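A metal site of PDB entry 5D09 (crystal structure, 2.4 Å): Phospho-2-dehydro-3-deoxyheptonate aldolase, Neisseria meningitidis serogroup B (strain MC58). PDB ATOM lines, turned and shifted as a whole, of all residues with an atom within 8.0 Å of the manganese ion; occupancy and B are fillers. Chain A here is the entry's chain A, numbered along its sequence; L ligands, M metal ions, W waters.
The side-chain hydroxyl (OG1) of Thr 323 sits close to the side-chain sulfur (SG) of Cys 63, 3.0 Å away.
N of Cys 63 sits at hydrogen-bond distance from SG of Cys 326 (3.5 Å).
The backbone carbonyl oxygen of Asp 324 is in hydrogen-bond range of the side-chain hydroxyl of Ser 321, 2.6 Å away.
The guanidinium group (NH2) of Arg 94 is in hydrogen-bond range of the backbone carbonyl oxygen (O) of Cys 63 (2.9 Å).
A ring nitrogen (ND1) of His 270 lies within hydrogen-bond range of the side-chain carboxylate (OD2) of Asp 267 (2.7 Å).
OD1 of Asp 324 lies within salt-bridge range of NZ of Lys 99 (2.9 Å).
The backbone carbonyl oxygen (O) of Asp 324 sits at hydrogen-bond distance from the side-chain sulfur (SG) of Cys 326 (3.7 Å).
OE2 of Glu 304 sits close to NH2 of Arg 94 (3.6 Å).
The side-chain amino group of Lys 188 is in salt-bridge range of an oxygen (O1) of the ligand, at 2.8 Å.
An oxygen (O2) of the ligand lies within salt-bridge range of the guanidinium group (NH2) of Arg 94 (2.5 Å).
Four residues have an atom within 4 Å of the manganese ion: Cys 63, His 270, Glu 304 and Asp 324.
The manganese ion is bound by water W1 (1.8 Å), OE2 of Glu 304 (1.9 Å), NE2 of His 270 (2.2 Å), OD2 of Asp 324 (2.3 Å) and SG of Cys 63 (2.5 Å).
The manganese ion has five donor atoms within binding distance.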
ATOM      1  N   GLY A  61     -10.918  26.341 -32.598  1.00  0.00           N
ATOM      2  CA  GLY A  61     -10.374  25.075 -32.177  1.00  0.00           C
ATOM      3  C   GLY A  61     -10.880  24.690 -30.793  1.00  0.00           C
ATOM      4  O   GLY A  61     -11.743  25.354 -30.261  1.00  0.00           O
ATOM      5  N   PRO A  62     -10.342  23.612 -30.233  1.00  0.00           N
ATOM      6  CA  PRO A  62     -10.742  23.138 -28.913  1.00  0.00           C
ATOM      7  C   PRO A  62     -10.597  24.176 -27.804  1.00  0.00           C
ATOM      8  O   PRO A  62      -9.688  24.996 -27.848  1.00  0.00           O
ATOM      9  CB  PRO A  62      -9.778  21.967 -28.695  1.00  0.00           C
ATOM     10  CG  PRO A  62      -9.528  21.449 -30.077  1.00  0.00           C
ATOM     11  CD  PRO A  62      -9.412  22.678 -30.895  1.00  0.00           C
ATOM     12  N   CYS A  63     -11.483  24.146 -26.813  1.00  0.00           N
ATOM     13  CA  CYS A  63     -11.273  24.947 -25.597  1.00  0.00           C
ATOM     14  C   CYS A  63      -9.882  24.635 -25.064  1.00  0.00           C
ATOM     15  O   CYS A  63      -9.133  25.535 -24.658  1.00  0.00           O
ATOM     16  CB  CYS A  63     -12.315  24.595 -24.527  1.00  0.00           C
ATOM     17  SG  CYS A  63     -12.048  25.448 -22.952  1.00  0.00           S
ATOM     18  N   SER A  64      -9.525  23.364 -25.051  1.00  0.00           N
ATOM     19  CA  SER A  64      -8.173  22.986 -24.640  1.00  0.00           C
ATOM     20  C   SER A  64      -7.737  21.730 -25.340  1.00  0.00           C
ATOM     21  O   SER A  64      -8.563  20.889 -25.748  1.00  0.00           O
ATOM     22  CB  SER A  64      -8.146  22.722 -23.133  1.00  0.00           C
ATOM     23  OG  SER A  64      -9.029  21.675 -22.823  1.00  0.00           O
ATOM     24  N   ARG A  94      -6.831  27.315 -32.435  1.00  0.00           N
ATOM     25  CA  ARG A  94      -6.729  27.374 -30.979  1.00  0.00           C
ATOM     26  C   ARG A  94      -5.895  26.204 -30.572  1.00  0.00           C
ATOM     27  O   ARG A  94      -6.274  25.066 -30.808  1.00  0.00           O
ATOM     28  CB  ARG A  94      -8.085  27.196 -30.260  1.00  0.00           C
ATOM     29  CG  ARG A  94      -8.832  28.467 -29.907  1.00  0.00           C
ATOM     30  CD  ARG A  94     -10.132  28.192 -29.172  1.00  0.00           C
ATOM     31  NE  ARG A  94      -9.916  27.824 -27.775  1.00  0.00           N
ATOM     32  CZ  ARG A  94      -9.921  28.668 -26.741  1.00  0.00           C
ATOM     33  NH1 ARG A  94     -10.196  29.960 -26.871  1.00  0.00           N
ATOM     34  NH2 ARG A  94      -9.682  28.193 -25.557  1.00  0.00           N
ATOM     35  N   TYR A  96      -4.665  25.856 -27.151  1.00  0.00           N
ATOM     36  CA  TYR A  96      -4.614  26.313 -25.785  1.00  0.00           C
ATOM     37  C   TYR A  96      -4.360  25.109 -24.961  1.00  0.00           C
ATOM     38  O   TYR A  96      -4.988  24.092 -25.170  1.00  0.00           O
ATOM     39  CB  TYR A  96      -5.968  26.886 -25.351  1.00  0.00           C
ATOM     40  CG  TYR A  96      -6.259  28.292 -25.773  1.00  0.00           C
ATOM     41  CD1 TYR A  96      -5.936  28.753 -27.046  1.00  0.00           C
ATOM     42  CD2 TYR A  96      -6.866  29.166 -24.913  1.00  0.00           C
ATOM     43  CE1 TYR A  96      -6.222  30.038 -27.424  1.00  0.00           C
ATOM     44  CE2 TYR A  96      -7.163  30.442 -25.290  1.00  0.00           C
ATOM     45  CZ  TYR A  96      -6.853  30.887 -26.550  1.00  0.00           C
ATOM     46  OH  TYR A  96      -7.159  32.176 -26.921  1.00  0.00           O
ATOM     47  N   GLU A  98      -4.692  24.749 -21.529  1.00  0.00           N
ATOM     48  CA  GLU A  98      -5.486  24.661 -20.300  1.00  0.00           C
ATOM     49  C   GLU A  98      -6.708  25.602 -20.323  1.00  0.00           C
ATOM     50  O   GLU A  98      -6.929  26.277 -21.306  1.00  0.00           O
ATOM     51  CB  GLU A  98      -4.618  24.942 -19.067  1.00  0.00           C
ATOM     52  CG  GLU A  98      -4.474  26.412 -18.731  1.00  0.00           C
ATOM     53  CD  GLU A  98      -4.096  26.636 -17.290  1.00  0.00           C
ATOM     54  OE1 GLU A  98      -3.038  26.132 -16.892  1.00  0.00           O
ATOM     55  OE2 GLU A  98      -4.850  27.316 -16.564  1.00  0.00           O
ATOM     56  N   LYS A  99      -7.620  25.386 -19.399  1.00  0.00           N
ATOM     57  CA  LYS A  99      -8.752  26.326 -19.191  1.00  0.00           C
ATOM     58  C   LYS A  99      -8.518  26.932 -17.814  1.00  0.00           C
ATOM     59  O   LYS A  99      -8.493  26.192 -16.825  1.00  0.00           O
ATOM     60  CB  LYS A  99     -10.126  25.621 -19.190  1.00  0.00           C
ATOM     61  CG  LYS A  99     -11.313  26.559 -18.890  1.00  0.00           C
ATOM     62  CD  LYS A  99     -12.562  25.822 -18.405  1.00  0.00           C
ATOM     63  CE  LYS A  99     -13.640  26.784 -17.848  1.00  0.00           C
ATOM     64  NZ  LYS A  99     -13.992  27.941 -18.750  1.00  0.00           N
ATOM     65  N   PRO A 100      -8.310  28.272 -17.740  1.00  0.00           N
ATOM     66  CA  PRO A 100      -7.919  28.763 -16.418  1.00  0.00           C
ATOM     67  C   PRO A 100      -8.992  28.440 -15.410  1.00  0.00           C
ATOM     68  O   PRO A 100     -10.180  28.296 -15.748  1.00  0.00           O
ATOM     69  CB  PRO A 100      -7.740  30.280 -16.608  1.00  0.00           C
ATOM     70  CG  PRO A 100      -7.430  30.427 -18.067  1.00  0.00           C
ATOM     71  CD  PRO A 100      -8.291  29.366 -18.732  1.00  0.00           C
ATOM     72  N   LYS A 188      -8.687  40.377 -23.418  1.00  0.00           N
ATOM     73  CA  LYS A 188     -10.126  40.219 -23.151  1.00  0.00           C
ATOM     74  C   LYS A 188     -10.648  41.254 -22.205  1.00  0.00           C
ATOM     75  O   LYS A 188      -9.937  41.616 -21.281  1.00  0.00           O
ATOM     76  CB  LYS A 188     -10.395  38.857 -22.554  1.00  0.00           C
ATOM     77  CG  LYS A 188     -10.017  37.759 -23.511  1.00  0.00           C
ATOM     78  CD  LYS A 188     -10.645  36.435 -23.188  1.00  0.00           C
ATOM     79  CE  LYS A 188     -10.993  35.751 -24.513  1.00  0.00           C
ATOM     80  NZ  LYS A 188     -11.604  34.407 -24.284  1.00  0.00           N
ATOM     81  N   ASP A 267     -15.588  37.012 -29.255  1.00  0.00           N
ATOM     82  CA  ASP A 267     -15.572  35.627 -28.888  1.00  0.00           C
ATOM     83  C   ASP A 267     -17.051  35.248 -28.930  1.00  0.00           C
ATOM     84  O   ASP A 267     -17.833  35.807 -28.197  1.00  0.00           O
ATOM     85  CB  ASP A 267     -14.959  35.462 -27.482  1.00  0.00           C
ATOM     86  CG  ASP A 267     -14.868  34.013 -26.991  1.00  0.00           C
ATOM     87  OD1 ASP A 267     -15.323  33.055 -27.656  1.00  0.00           O
ATOM     88  OD2 ASP A 267     -14.315  33.818 -25.881  1.00  0.00           O
ATOM     89  N   SER A 269     -17.956  32.396 -27.912  1.00  0.00           N
ATOM     90  CA  SER A 269     -18.121  31.386 -26.842  1.00  0.00           C
ATOM     91  C   SER A 269     -18.078  32.050 -25.476  1.00  0.00           C
ATOM     92  O   SER A 269     -18.295  33.292 -25.376  1.00  0.00           O
ATOM     93  CB  SER A 269     -17.010  30.329 -26.958  1.00  0.00           C
ATOM     94  OG  SER A 269     -17.322  29.090 -26.309  1.00  0.00           O
ATOM     95  N   HIS A 270     -17.821  31.253 -24.427  1.00  0.00           N
ATOM     96  CA  HIS A 270     -17.753  31.728 -23.022  1.00  0.00           C
ATOM     97  C   HIS A 270     -18.937  32.618 -22.652  1.00  0.00           C
ATOM     98  O   HIS A 270     -20.079  32.210 -22.910  1.00  0.00           O
ATOM     99  CB  HIS A 270     -16.401  32.362 -22.753  1.00  0.00           C
ATOM    100  CG  HIS A 270     -15.269  31.449 -23.096  1.00  0.00           C
ATOM    101  ND1 HIS A 270     -14.485  31.637 -24.222  1.00  0.00           N
ATOM    102  CD2 HIS A 270     -14.853  30.283 -22.541  1.00  0.00           C
ATOM    103  CE1 HIS A 270     -13.606  30.661 -24.300  1.00  0.00           C
ATOM    104  NE2 HIS A 270     -13.804  29.822 -23.297  1.00  0.00           N
ATOM    105  N   MET A 302     -13.599  34.438 -32.439  1.00  0.00           N
ATOM    106  CA  MET A 302     -13.090  33.307 -31.689  1.00  0.00           C
ATOM    107  C   MET A 302     -14.179  32.262 -31.543  1.00  0.00           C
ATOM    108  O   MET A 302     -15.310  32.586 -31.176  1.00  0.00           O
ATOM    109  CB  MET A 302     -12.649  33.779 -30.313  1.00  0.00           C
ATOM    110  CG  MET A 302     -11.758  32.827 -29.529  1.00  0.00           C
ATOM    111  SD  MET A 302     -10.970  33.551 -28.037  1.00  0.00           S
ATOM    112  CE  MET A 302     -10.550  35.185 -28.637  1.00  0.00           C
ATOM    113  N   GLU A 304     -15.045  28.066 -30.155  1.00  0.00           N
ATOM    114  CA  GLU A 304     -14.601  26.836 -29.502  1.00  0.00           C
ATOM    115  C   GLU A 304     -15.176  25.597 -30.206  1.00  0.00           C
ATOM    116  O   GLU A 304     -16.364  25.322 -30.181  1.00  0.00           O
ATOM    117  CB  GLU A 304     -14.901  26.879 -28.008  1.00  0.00           C
ATOM    118  CG  GLU A 304     -13.907  27.743 -27.226  1.00  0.00           C
ATOM    119  CD  GLU A 304     -14.157  27.716 -25.734  1.00  0.00           C
ATOM    120  OE1 GLU A 304     -15.321  27.819 -25.340  1.00  0.00           O
ATOM    121  OE2 GLU A 304     -13.215  27.593 -24.946  1.00  0.00           O
ATOM    122  N   SER A 321     -14.079  17.621 -26.180  1.00  0.00           N
ATOM    123  CA  SER A 321     -13.514  18.455 -25.114  1.00  0.00           C
ATOM    124  C   SER A 321     -13.728  17.916 -23.713  1.00  0.00           C
ATOM    125  O   SER A 321     -14.775  17.356 -23.406  1.00  0.00           O
ATOM    126  CB  SER A 321     -14.168  19.845 -25.142  1.00  0.00           C
ATOM    127  OG  SER A 321     -13.545  20.716 -24.204  1.00  0.00           O
ATOM    128  N   THR A 323     -12.757  20.351 -21.229  1.00  0.00           N
ATOM    129  CA  THR A 323     -12.983  21.602 -20.516  1.00  0.00           C
ATOM    130  C   THR A 323     -14.324  22.146 -20.991  1.00  0.00           C
ATOM    131  O   THR A 323     -15.311  21.435 -20.892  1.00  0.00           O
ATOM    132  CB  THR A 323     -11.802  22.534 -20.700  1.00  0.00           C
ATOM    133  OG1 THR A 323     -11.452  22.631 -22.092  1.00  0.00           O
ATOM    134  CG2 THR A 323     -10.628  21.987 -19.893  1.00  0.00           C
ATOM    135  N   ASP A 324     -14.381  23.348 -21.552  1.00  0.00           N
ATOM    136  CA  ASP A 324     -15.665  23.867 -22.043  1.00  0.00           C
ATOM    137  C   ASP A 324     -16.133  23.099 -23.245  1.00  0.00           C
ATOM    138  O   ASP A 324     -15.358  22.551 -24.029  1.00  0.00           O
ATOM    139  CB  ASP A 324     -15.642  25.353 -22.375  1.00  0.00           C
ATOM    140  CG  ASP A 324     -15.278  26.210 -21.185  1.00  0.00           C
ATOM    141  OD1 ASP A 324     -15.600  25.834 -20.019  1.00  0.00           O
ATOM    142  OD2 ASP A 324     -14.673  27.266 -21.416  1.00  0.00           O
ATOM    143  N   ALA A 325     -17.444  23.030 -23.339  1.00  0.00           N
ATOM    144  CA  ALA A 325     -18.098  22.345 -24.384  1.00  0.00           C
ATOM    145  C   ALA A 325     -17.853  23.079 -25.695  1.00  0.00           C
ATOM    146  O   ALA A 325     -17.836  24.310 -25.759  1.00  0.00           O
ATOM    147  CB  ALA A 325     -19.589  22.329 -24.072  1.00  0.00           C
ATOM    148  N   CYS A 326     -17.678  22.316 -26.762  1.00  0.00           N
ATOM    149  CA  CYS A 326     -17.433  22.884 -28.074  1.00  0.00           C
ATOM    150  C   CYS A 326     -18.498  22.464 -29.039  1.00  0.00           C
ATOM    151  O   CYS A 326     -19.161  21.440 -28.839  1.00  0.00           O
ATOM    152  CB  CYS A 326     -16.101  22.364 -28.572  1.00  0.00           C
ATOM    153  SG  CYS A 326     -14.683  22.957 -27.640  1.00  0.00           S
HETATM  154  C1  LIG L   1     -10.539  31.082 -23.688  1.00  0.00           C
HETATM  155  O1  LIG L   1     -10.555  31.867 -24.673  1.00  0.00           O
HETATM  156  O2  LIG L   1     -10.324  29.874 -23.892  1.00  0.00           O
HETATM  157  C2  LIG L   1     -10.805  31.554 -22.303  1.00  0.00           C
HETATM  158  C3  LIG L   1     -10.271  30.922 -21.270  1.00  0.00           C
HETATM  159  O3  LIG L   1     -11.697  32.709 -22.143  1.00  0.00           O
HETATM  160  P1  LIG L   1     -11.748  33.714 -20.867  1.00  0.00           P
HETATM  161  O4  LIG L   1     -10.315  34.203 -20.640  1.00  0.00           O
HETATM  162  O5  LIG L   1     -12.736  34.710 -21.413  1.00  0.00           O
HETATM  163  O6  LIG L   1     -12.335  32.857 -19.735  1.00  0.00           O
HETATM  164 MN    MN M   1     -13.102  27.727 -23.041  1.00  0.00          MN
HETATM  165  O   HOH W   1     -11.714  28.315 -21.991  1.00  0.00           O
